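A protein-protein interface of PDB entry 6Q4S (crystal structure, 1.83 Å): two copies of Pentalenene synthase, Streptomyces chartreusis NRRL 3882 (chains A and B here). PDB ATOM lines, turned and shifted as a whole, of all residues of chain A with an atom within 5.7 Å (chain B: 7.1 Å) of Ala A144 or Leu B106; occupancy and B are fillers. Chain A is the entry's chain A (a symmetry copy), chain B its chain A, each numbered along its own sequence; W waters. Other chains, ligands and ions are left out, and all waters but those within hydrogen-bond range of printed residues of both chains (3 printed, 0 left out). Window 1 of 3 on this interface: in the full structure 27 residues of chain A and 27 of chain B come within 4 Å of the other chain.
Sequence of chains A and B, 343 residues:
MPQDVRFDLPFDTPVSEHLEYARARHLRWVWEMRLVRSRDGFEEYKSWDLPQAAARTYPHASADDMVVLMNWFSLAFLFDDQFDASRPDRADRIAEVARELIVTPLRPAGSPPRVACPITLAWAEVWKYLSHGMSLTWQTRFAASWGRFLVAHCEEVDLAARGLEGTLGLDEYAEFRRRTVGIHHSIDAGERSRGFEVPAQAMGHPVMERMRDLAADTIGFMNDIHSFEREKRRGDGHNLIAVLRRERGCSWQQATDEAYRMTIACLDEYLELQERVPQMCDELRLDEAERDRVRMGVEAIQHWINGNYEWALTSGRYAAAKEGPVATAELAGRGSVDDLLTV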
ATOM      1  N   ILE A 102      -5.941 -19.395  20.225  1.00  0.00           N
ATOM      2  CA  ILE A 102      -5.697 -18.643  21.430  1.00  0.00           C
ATOM      3  C   ILE A 102      -6.815 -17.605  21.650  1.00  0.00           C
ATOM      4  O   ILE A 102      -7.264 -17.407  22.778  1.00  0.00           O
ATOM      5  CB  ILE A 102      -4.300 -17.929  21.414  1.00  0.00           C
ATOM      6  CG1 ILE A 102      -3.222 -18.992  21.519  1.00  0.00           C
ATOM      7  CG2 ILE A 102      -4.162 -16.933  22.580  1.00  0.00           C
ATOM      8  CD1 ILE A 102      -1.802 -18.508  21.256  1.00  0.00           C
ATOM      9  N   LEU A 106     -11.116 -15.880  24.133  1.00  0.00           N
ATOM     10  CA  LEU A 106     -11.133 -14.459  24.527  1.00  0.00           C
ATOM     11  C   LEU A 106     -12.219 -13.660  23.805  1.00  0.00           C
ATOM     12  O   LEU A 106     -12.141 -12.444  23.692  1.00  0.00           O
ATOM     13  CB  LEU A 106      -9.733 -13.866  24.230  1.00  0.00           C
ATOM     14  CG  LEU A 106      -8.646 -14.525  25.108  1.00  0.00           C
ATOM     15  CD1 LEU A 106      -7.274 -14.061  24.629  1.00  0.00           C
ATOM     16  CD2 LEU A 106      -8.860 -14.268  26.597  1.00  0.00           C
ATOM     17  N   GLN A 139     -12.819 -19.243  33.280  1.00  0.00           N
ATOM     18  CA  GLN A 139     -12.584 -19.028  31.868  1.00  0.00           C
ATOM     19  C   GLN A 139     -11.284 -18.232  31.637  1.00  0.00           C
ATOM     20  O   GLN A 139     -10.557 -18.515  30.679  1.00  0.00           O
ATOM     21  CB  GLN A 139     -13.774 -18.309  31.211  1.00  0.00           C
ATOM     22  CG  GLN A 139     -15.015 -19.140  31.219  1.00  0.00           C
ATOM     23  CD  GLN A 139     -16.200 -18.391  30.621  1.00  0.00           C
ATOM     24  OE1 GLN A 139     -16.088 -17.893  29.544  1.00  0.00           O
ATOM     25  NE2 GLN A 139     -17.302 -18.353  31.297  1.00  0.00           N
ATOM     26  N   THR A 140     -11.019 -17.273  32.481  1.00  0.00           N
ATOM     27  CA  THR A 140      -9.768 -16.473  32.407  1.00  0.00           C
ATOM     28  C   THR A 140      -8.542 -17.323  32.677  1.00  0.00           C
ATOM     29  O   THR A 140      -7.588 -17.275  31.935  1.00  0.00           O
ATOM     30  CB  THR A 140      -9.825 -15.349  33.422  1.00  0.00           C
ATOM     31  OG1 THR A 140     -10.788 -14.393  32.965  1.00  0.00           O
ATOM     32  CG2 THR A 140      -8.491 -14.680  33.626  1.00  0.00           C
ATOM     33  N   ARG A 141      -8.607 -18.105  33.749  1.00  0.00           N
ATOM     34  CA  ARG A 141      -7.560 -19.032  34.086  1.00  0.00           C
ATOM     35  C   ARG A 141      -7.303 -20.037  32.946  1.00  0.00           C
ATOM     36  O   ARG A 141      -6.148 -20.221  32.558  1.00  0.00           O
ATOM     37  CB  ARG A 141      -7.859 -19.716  35.426  1.00  0.00           C
ATOM     38  CG  ARG A 141      -6.985 -20.932  35.718  1.00  0.00           C
ATOM     39  CD  ARG A 141      -6.770 -21.166  37.210  1.00  0.00           C
ATOM     40  NE  ARG A 141      -8.015 -21.344  37.952  1.00  0.00           N
ATOM     41  CZ  ARG A 141      -8.788 -22.432  37.966  1.00  0.00           C
ATOM     42  NH1 ARG A 141      -9.941 -22.414  38.692  1.00  0.00           N
ATOM     43  NH2 ARG A 141      -8.486 -23.513  37.260  1.00  0.00           N
ATOM     44  N   PHE A 142      -8.361 -20.676  32.433  1.00  0.00           N
ATOM     45  CA  PHE A 142      -8.257 -21.621  31.316  1.00  0.00           C
ATOM     46  C   PHE A 142      -7.624 -20.938  30.100  1.00  0.00           C
ATOM     47  O   PHE A 142      -6.701 -21.466  29.437  1.00  0.00           O
ATOM     48  CB  PHE A 142      -9.585 -22.255  30.918  1.00  0.00           C
ATOM     49  CG  PHE A 142      -9.443 -23.213  29.744  1.00  0.00           C
ATOM     50  CD1 PHE A 142      -9.458 -22.761  28.436  1.00  0.00           C
ATOM     51  CD2 PHE A 142      -9.237 -24.535  29.962  1.00  0.00           C
ATOM     52  CE1 PHE A 142      -9.221 -23.623  27.365  1.00  0.00           C
ATOM     53  CE2 PHE A 142      -9.053 -25.427  28.917  1.00  0.00           C
ATOM     54  CZ  PHE A 142      -9.042 -24.974  27.602  1.00  0.00           C
ATOM     55  N   ALA A 143      -8.117 -19.758  29.807  1.00  0.00           N
ATOM     56  CA  ALA A 143      -7.715 -19.069  28.614  1.00  0.00           C
ATOM     57  C   ALA A 143      -6.208 -18.748  28.650  1.00  0.00           C
ATOM     58  O   ALA A 143      -5.491 -18.863  27.656  1.00  0.00           O
ATOM     59  CB  ALA A 143      -8.516 -17.795  28.435  1.00  0.00           C
ATOM     60  N   ALA A 144      -5.726 -18.340  29.793  1.00  0.00           N
ATOM     61  CA  ALA A 144      -4.286 -18.044  29.836  1.00  0.00           C
ATOM     62  C   ALA A 144      -3.488 -19.352  29.819  1.00  0.00           C
ATOM     63  O   ALA A 144      -2.504 -19.416  29.161  1.00  0.00           O
ATOM     64  CB  ALA A 144      -3.971 -17.230  31.077  1.00  0.00           C
ATOM     65  N   SER A 145      -3.902 -20.390  30.546  1.00  0.00           N
ATOM     66  CA  SER A 145      -3.191 -21.670  30.527  1.00  0.00           C
ATOM     67  C   SER A 145      -3.053 -22.242  29.082  1.00  0.00           C
ATOM     68  O   SER A 145      -1.966 -22.598  28.614  1.00  0.00           O
ATOM     69  CB  SER A 145      -3.890 -22.712  31.431  1.00  0.00           C
ATOM     70  OG  SER A 145      -3.850 -22.409  32.803  1.00  0.00           O
ATOM     71  N   TRP A 146      -4.171 -22.288  28.376  1.00  0.00           N
ATOM     72  CA  TRP A 146      -4.269 -22.758  26.993  1.00  0.00           C
ATOM     73  C   TRP A 146      -3.406 -21.899  26.057  1.00  0.00           C
ATOM     74  O   TRP A 146      -2.693 -22.411  25.203  1.00  0.00           O
ATOM     75  CB  TRP A 146      -5.724 -22.631  26.569  1.00  0.00           C
ATOM     76  CG  TRP A 146      -6.097 -22.976  25.141  1.00  0.00           C
ATOM     77  CD1 TRP A 146      -6.596 -22.096  24.215  1.00  0.00           C
ATOM     78  CD2 TRP A 146      -6.152 -24.258  24.513  1.00  0.00           C
ATOM     79  NE1 TRP A 146      -6.883 -22.734  23.071  1.00  0.00           N
ATOM     80  CE2 TRP A 146      -6.625 -24.052  23.200  1.00  0.00           C
ATOM     81  CE3 TRP A 146      -5.791 -25.560  24.899  1.00  0.00           C
ATOM     82  CZ2 TRP A 146      -6.790 -25.086  22.275  1.00  0.00           C
ATOM     83  CZ3 TRP A 146      -5.995 -26.602  23.983  1.00  0.00           C
ATOM     84  CH2 TRP A 146      -6.450 -26.338  22.676  1.00  0.00           C
ATOM     85  N   GLY A 147      -3.526 -20.591  26.233  1.00  0.00           N
ATOM     86  CA  GLY A 147      -2.691 -19.644  25.488  1.00  0.00           C
ATOM     87  C   GLY A 147      -1.201 -19.817  25.684  1.00  0.00           C
ATOM     88  O   GLY A 147      -0.442 -19.832  24.697  1.00  0.00           O
ATOM     89  N   ARG A 148      -0.773 -19.972  26.928  1.00  0.00           N
ATOM     90  CA  ARG A 148       0.675 -20.193  27.209  1.00  0.00           C
ATOM     91  C   ARG A 148       1.161 -21.489  26.516  1.00  0.00           C
ATOM     92  O   ARG A 148       2.209 -21.508  25.883  1.00  0.00           O
ATOM     93  CB  ARG A 148       0.947 -20.276  28.712  1.00  0.00           C
ATOM     94  CG  ARG A 148       0.746 -18.975  29.471  1.00  0.00           C
ATOM     95  CD  ARG A 148       1.127 -19.094  30.929  1.00  0.00           C
ATOM     96  NE  ARG A 148       0.738 -17.799  31.597  1.00  0.00           N
ATOM     97  CZ  ARG A 148      -0.309 -17.617  32.360  1.00  0.00           C
ATOM     98  NH1 ARG A 148      -1.057 -18.675  32.713  1.00  0.00           N
ATOM     99  NH2 ARG A 148      -0.598 -16.385  32.788  1.00  0.00           N
ATOM    100  N   PHE A 149       0.324 -22.531  26.552  1.00  0.00           N
ATOM    101  CA  PHE A 149       0.578 -23.777  25.892  1.00  0.00           C
ATOM    102  C   PHE A 149       0.771 -23.591  24.399  1.00  0.00           C
ATOM    103  O   PHE A 149       1.720 -24.131  23.779  1.00  0.00           O
ATOM    104  CB  PHE A 149      -0.549 -24.821  26.192  1.00  0.00           C
ATOM    105  CG  PHE A 149      -0.613 -25.914  25.199  1.00  0.00           C
ATOM    106  CD1 PHE A 149       0.429 -26.823  25.108  1.00  0.00           C
ATOM    107  CD2 PHE A 149      -1.673 -26.014  24.298  1.00  0.00           C
ATOM    108  CE1 PHE A 149       0.366 -27.881  24.209  1.00  0.00           C
ATOM    109  CE2 PHE A 149      -1.714 -27.026  23.354  1.00  0.00           C
ATOM    110  CZ  PHE A 149      -0.659 -27.978  23.326  1.00  0.00           C
ATOM    111  N   VAL A 151       1.419 -20.848  22.609  1.00  0.00           N
ATOM    112  CA  VAL A 151       2.580 -20.041  22.307  1.00  0.00           C
ATOM    113  C   VAL A 151       3.858 -20.916  22.321  1.00  0.00           C
ATOM    114  O   VAL A 151       4.665 -20.880  21.384  1.00  0.00           O
ATOM    115  CB  VAL A 151       2.729 -18.871  23.277  1.00  0.00           C
ATOM    116  CG1 VAL A 151       4.109 -18.178  23.069  1.00  0.00           C
ATOM    117  CG2 VAL A 151       1.585 -17.834  23.069  1.00  0.00           C
ATOM    118  N   ARG A 179       6.356 -25.873  29.773  1.00  0.00           N
ATOM    119  CA  ARG A 179       5.437 -25.069  28.983  1.00  0.00           C
ATOM    120  C   ARG A 179       4.747 -25.876  27.873  1.00  0.00           C
ATOM    121  O   ARG A 179       3.567 -25.731  27.668  1.00  0.00           O
ATOM    122  CB  ARG A 179       6.128 -23.853  28.401  1.00  0.00           C
ATOM    123  CG  ARG A 179       6.865 -22.955  29.443  1.00  0.00           C
ATOM    124  CD  ARG A 179       7.761 -21.923  28.758  1.00  0.00           C
ATOM    125  NE  ARG A 179       7.057 -21.104  27.771  1.00  0.00           N
ATOM    126  CZ  ARG A 179       7.588 -20.615  26.665  1.00  0.00           C
ATOM    127  NH1 ARG A 179       8.859 -20.876  26.336  1.00  0.00           N
ATOM    128  NH2 ARG A 179       6.839 -19.950  25.797  1.00  0.00           N
ATOM    129  N   LEU B 101       0.377  -8.726  20.067  1.00  0.00           N
ATOM    130  CA  LEU B 101       0.186  -8.042  21.352  1.00  0.00           C
ATOM    131  C   LEU B 101      -0.569  -8.905  22.376  1.00  0.00           C
ATOM    132  O   LEU B 101      -0.299  -8.879  23.594  1.00  0.00           O
ATOM    133  CB  LEU B 101      -0.499  -6.715  21.114  1.00  0.00           C
ATOM    134  CG  LEU B 101       0.112  -5.704  20.113  1.00  0.00           C
ATOM    135  CD1 LEU B 101      -0.818  -4.485  20.028  1.00  0.00           C
ATOM    136  CD2 LEU B 101       1.481  -5.326  20.591  1.00  0.00           C
ATOM    137  N   ILE B 102      -1.468  -9.747  21.887  1.00  0.00           N
ATOM    138  CA  ILE B 102      -2.201 -10.630  22.759  1.00  0.00           C
ATOM    139  C   ILE B 102      -1.268 -11.718  23.329  1.00  0.00           C
ATOM    140  O   ILE B 102      -1.363 -12.061  24.506  1.00  0.00           O
ATOM    141  CB  ILE B 102      -3.424 -11.298  22.038  1.00  0.00           C
ATOM    142  CG1 ILE B 102      -4.466 -10.225  21.779  1.00  0.00           C
ATOM    143  CG2 ILE B 102      -4.039 -12.421  22.893  1.00  0.00           C
ATOM    144  CD1 ILE B 102      -5.605 -10.634  20.855  1.00  0.00           C
ATOM    145  N   VAL B 103      -0.378 -12.280  22.534  1.00  0.00           N
ATOM    146  CA  VAL B 103       0.408 -13.409  23.066  1.00  0.00           C
ATOM    147  C   VAL B 103       1.593 -12.970  23.900  1.00  0.00           C
ATOM    148  O   VAL B 103       2.137 -13.752  24.609  1.00  0.00           O
ATOM    149  CB  VAL B 103       0.852 -14.368  21.970  1.00  0.00           C
ATOM    150  CG1 VAL B 103      -0.343 -14.918  21.224  1.00  0.00           C
ATOM    151  CG2 VAL B 103       1.758 -13.752  20.957  1.00  0.00           C
ATOM    152  N   THR B 104       1.978 -11.695  23.853  1.00  0.00           N
ATOM    153  CA  THR B 104       3.196 -11.223  24.555  1.00  0.00           C
ATOM    154  C   THR B 104       3.058 -11.469  26.041  1.00  0.00           C
ATOM    155  O   THR B 104       3.991 -11.979  26.666  1.00  0.00           O
ATOM    156  CB  THR B 104       3.502  -9.758  24.152  1.00  0.00           C
ATOM    157  OG1 THR B 104       4.023  -9.755  22.821  1.00  0.00           O
ATOM    158  CG2 THR B 104       4.463  -9.071  25.077  1.00  0.00           C
ATOM    159  N   PRO B 105       1.873 -11.210  26.633  1.00  0.00           N
ATOM    160  CA  PRO B 105       1.769 -11.565  28.048  1.00  0.00           C
ATOM    161  C   PRO B 105       1.575 -13.028  28.302  1.00  0.00           C
ATOM    162  O   PRO B 105       1.553 -13.422  29.449  1.00  0.00           O
ATOM    163  CB  PRO B 105       0.530 -10.826  28.524  1.00  0.00           C
ATOM    164  CG  PRO B 105       0.323  -9.736  27.511  1.00  0.00           C
ATOM    165  CD  PRO B 105       0.788 -10.317  26.219  1.00  0.00           C
ATOM    166  N   LEU B 106       1.524 -13.846  27.241  1.00  0.00           N
ATOM    167  CA  LEU B 106       1.404 -15.303  27.429  1.00  0.00           C
ATOM    168  C   LEU B 106       2.720 -16.041  27.176  1.00  0.00           C
ATOM    169  O   LEU B 106       2.734 -17.232  26.896  1.00  0.00           O
ATOM    170  CB  LEU B 106       0.300 -15.818  26.472  1.00  0.00           C
ATOM    171  CG  LEU B 106      -1.083 -15.238  26.847  1.00  0.00           C
ATOM    172  CD1 LEU B 106      -2.084 -15.603  25.755  1.00  0.00           C
ATOM    173  CD2 LEU B 106      -1.545 -15.675  28.232  1.00  0.00           C
ATOM    174  N   ARG B 107       3.828 -15.329  27.258  1.00  0.00           N
ATOM    175  CA  ARG B 107       5.153 -15.921  27.008  1.00  0.00           C
ATOM    176  C   ARG B 107       6.145 -15.260  28.028  1.00  0.00           C
ATOM    177  O   ARG B 107       5.829 -14.204  28.580  1.00  0.00           O
ATOM    178  CB  ARG B 107       5.463 -15.695  25.516  1.00  0.00           C
ATOM    179  CG  ARG B 107       6.587 -14.795  25.181  1.00  0.00           C
ATOM    180  CD  ARG B 107       6.455 -13.837  24.040  1.00  0.00           C
ATOM    181  NE  ARG B 107       6.106 -14.329  22.757  1.00  0.00           N
ATOM    182  CZ  ARG B 107       5.691 -13.515  21.794  1.00  0.00           C
ATOM    183  NH1 ARG B 107       5.654 -12.175  21.947  1.00  0.00           N
ATOM    184  NH2 ARG B 107       5.323 -14.042  20.656  1.00  0.00           N
ATOM    185  N   PRO B 108       7.292 -15.893  28.326  1.00  0.00           N
ATOM    186  CA  PRO B 108       8.119 -15.301  29.386  1.00  0.00           C
ATOM    187  C   PRO B 108       8.558 -13.853  29.066  1.00  0.00           C
ATOM    188  O   PRO B 108       8.745 -13.478  27.926  1.00  0.00           O
ATOM    189  CB  PRO B 108       9.308 -16.265  29.479  1.00  0.00           C
ATOM    190  CG  PRO B 108       8.665 -17.574  29.139  1.00  0.00           C
ATOM    191  CD  PRO B 108       7.803 -17.235  27.951  1.00  0.00           C
ATOM    192  N   TRP B 127       5.690  -4.770  28.762  1.00  0.00           N
ATOM    193  CA  TRP B 127       5.104  -5.878  29.525  1.00  0.00           C
ATOM    194  C   TRP B 127       6.080  -6.435  30.558  1.00  0.00           C
ATOM    195  O   TRP B 127       5.703  -6.713  31.650  1.00  0.00           O
ATOM    196  CB  TRP B 127       4.610  -7.021  28.608  1.00  0.00           C
ATOM    197  CG  TRP B 127       4.239  -8.245  29.379  1.00  0.00           C
ATOM    198  CD1 TRP B 127       4.909  -9.422  29.405  1.00  0.00           C
ATOM    199  CD2 TRP B 127       3.168  -8.379  30.307  1.00  0.00           C
ATOM    200  NE1 TRP B 127       4.319 -10.301  30.272  1.00  0.00           N
ATOM    201  CE2 TRP B 127       3.234  -9.686  30.838  1.00  0.00           C
ATOM    202  CE3 TRP B 127       2.169  -7.526  30.758  1.00  0.00           C
ATOM    203  CZ2 TRP B 127       2.328 -10.162  31.761  1.00  0.00           C
ATOM    204  CZ3 TRP B 127       1.294  -8.000  31.700  1.00  0.00           C
ATOM    205  CH2 TRP B 127       1.349  -9.322  32.153  1.00  0.00           C
ATOM    206  N   LEU B 136       1.370 -14.550  39.413  1.00  0.00           N
ATOM    207  CA  LEU B 136       0.826 -15.281  38.294  1.00  0.00           C
ATOM    208  C   LEU B 136      -0.721 -15.040  38.148  1.00  0.00           C
ATOM    209  O   LEU B 136      -1.230 -14.899  37.037  1.00  0.00           O
ATOM    210  CB  LEU B 136       1.146 -16.791  38.408  1.00  0.00           C
ATOM    211  CG  LEU B 136       0.685 -17.606  37.171  1.00  0.00           C
ATOM    212  CD1 LEU B 136       1.440 -17.156  35.916  1.00  0.00           C
ATOM    213  CD2 LEU B 136       0.919 -19.077  37.458  1.00  0.00           C
ATOM    214  N   GLN B 139      -1.115 -11.644  36.518  1.00  0.00           N
ATOM    215  CA  GLN B 139      -0.692 -11.683  35.134  1.00  0.00           C
ATOM    216  C   GLN B 139      -1.729 -12.409  34.256  1.00  0.00           C
ATOM    217  O   GLN B 139      -1.962 -11.994  33.116  1.00  0.00           O
ATOM    218  CB  GLN B 139       0.687 -12.352  34.995  1.00  0.00           C
ATOM    219  CG  GLN B 139       1.770 -11.562  35.653  1.00  0.00           C
ATOM    220  CD  GLN B 139       3.118 -12.268  35.560  1.00  0.00           C
ATOM    221  OE1 GLN B 139       3.511 -12.631  34.495  1.00  0.00           O
ATOM    222  NE2 GLN B 139       3.805 -12.417  36.647  1.00  0.00           N
ATOM    223  N   THR B 140      -2.315 -13.454  34.773  1.00  0.00           N
ATOM    224  CA  THR B 140      -3.380 -14.204  34.055  1.00  0.00           C
ATOM    225  C   THR B 140      -4.622 -13.358  33.850  1.00  0.00           C
ATOM    226  O   THR B 140      -5.143 -13.290  32.763  1.00  0.00           O
ATOM    227  CB  THR B 140      -3.749 -15.442  34.849  1.00  0.00           C
ATOM    228  OG1 THR B 140      -2.657 -16.363  34.757  1.00  0.00           O
ATOM    229  CG2 THR B 140      -5.015 -16.092  34.356  1.00  0.00           C
ATOM    230  N   ARG B 141      -5.062 -12.711  34.925  1.00  0.00           N
ATOM    231  CA  ARG B 141      -6.175 -11.802  34.868  1.00  0.00           C
ATOM    232  C   ARG B 141      -5.926 -10.661  33.862  1.00  0.00           C
ATOM    233  O   ARG B 141      -6.793 -10.401  33.024  1.00  0.00           O
ATOM    234  CB  ARG B 141      -6.523 -11.291  36.272  1.00  0.00           C
ATOM    235  CG  ARG B 141      -7.470 -10.094  36.287  1.00  0.00           C
ATOM    236  CD  ARG B 141      -8.333 -10.033  37.543  1.00  0.00           C
ATOM    237  NE  ARG B 141      -7.553  -9.979  38.777  1.00  0.00           N
ATOM    238  CZ  ARG B 141      -6.897  -8.923  39.263  1.00  0.00           C
ATOM    239  NH1 ARG B 141      -6.188  -9.059  40.417  1.00  0.00           N
ATOM    240  NH2 ARG B 141      -6.884  -7.758  38.630  1.00  0.00           N
ATOM    241  N   ALA B 143      -3.794 -10.588  31.404  1.00  0.00           N
ATOM    242  CA  ALA B 143      -3.603 -11.119  30.084  1.00  0.00           C
ATOM    243  C   ALA B 143      -4.958 -11.399  29.408  1.00  0.00           C
ATOM    244  O   ALA B 143      -5.162 -11.146  28.221  1.00  0.00           O
ATOM    245  CB  ALA B 143      -2.771 -12.384  30.130  1.00  0.00           C
ATOM    246  N   ALA B 144      -5.888 -11.926  30.159  1.00  0.00           N
ATOM    247  CA  ALA B 144      -7.188 -12.185  29.522  1.00  0.00           C
ATOM    248  C   ALA B 144      -7.931 -10.862  29.307  1.00  0.00           C
ATOM    249  O   ALA B 144      -8.521 -10.693  28.293  1.00  0.00           O
ATOM    250  CB  ALA B 144      -7.998 -13.132  30.385  1.00  0.00           C
HETATM  251  O   HOH W   1       0.215 -13.872  31.801  1.00  0.00           O
HETATM  252  O   HOH W   2       2.617 -15.716  30.696  1.00  0.00           O
HETATM  253  O   HOH W   3       4.075 -19.464  26.705  1.00  0.00           O
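Ala A144 touches two residues of chain B.
Leu B106 touches just these residues of chain A: Ala A144, Arg A148 and Val A151.
Of the printed residues of chain A, Pro B108 touches Arg A179.
Printed residues of chain B within 4 Å of Leu A106: Ala B144.
Ala A143 touches none of the printed residues of chain B.
Water W3 lies within hydrogen-bond range of the backbone carbonyl oxygen (O) of Leu B106, the backbone carbonyl oxygen (O) of Arg A148 and the guanidinium group (NH2) of Arg A179.
Water W1 lies within hydrogen-bond range of O of Pro B105 (2.7 Å), NH2 of Arg A148 (2.8 Å) and O of Gln B139 (3.2 Å).
Water W2 bridges the backbone carbonyl oxygen of Pro B105 and the guanidinium group of Arg A148.
Leu A106 touches Ala B144, and with the chains exchanged Ala A144 touches Leu B106.
Thr A140 touches its own counterpart, Thr B140.
Thr A140 touches Arg B141, and with the chains exchanged Arg A141 touches Thr B140.
Thr A140 touches Ala B144, and with the chains exchanged Ala A144 touches Thr B140.
Positions printed for both chains: 102, 106, 139, 140, 141, 143 and 144.
The side-chain hydroxyl of Thr B104 sits at hydrogen-bond distance from the guanidinium group of Arg B107 (3.0 Å).
The backbone carbonyl oxygen (O) of Leu B136 sits at hydrogen-bond distance from the side-chain hydroxyl (OG1) of Thr B140 (3.1 Å).
O of Arg A141 sits at hydrogen-bond distance from OG of Ser A145 (3.2 Å).
Among the printed residues, merely in contact across the chains: Arg A179 with Pro B108 (3.6 Å), Arg A148 with Leu B106 (3.6 Å), Ala A144 with Thr B140 (3.6 Å), Thr A140 with Ala B144 (3.6 Å), Val A151 with Val B103 (3.7 Å), Thr A140 with Thr B140 (3.7 Å), Val A151 with Arg B107 (3.7 Å), Arg A148 with Leu B136 (3.8 Å), Ile A102 with Val B103 (3.9 Å), Thr A140 with Arg B141 (3.9 Å), Arg A141 with Thr B140 (3.9 Å), Leu A106 with Ala B144 (3.96 Å), Ala A144 with Leu B106 (3.96 Å) and Val A151 with Leu B106 (3.97 Å).
The side-chain hydroxyl (OG1) of Thr B140 is in hydrogen-bond range of the guanidinium group (NH2) of Arg A148 (2.8 Å).
Of the 15 printed residues of chain B, 8 touch a printed residue of chain A.
Printed residues of chain B that touch a printed residue of chain A: Val B103, Leu B106, Arg B107, Pro B108, Leu B136, Thr B140, Arg B141 and Ala B144.
Hydrophobic or aromatic side chains of chain B that line the printed part of chain A: Val B103, Leu B106, Pro B108, Leu B136 and Ala B144.
Hydrophobic or aromatic side chains of chain A within 4 Å of the printed part of chain B: Ile A102, Leu A106, Ala A144 and Val A151.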
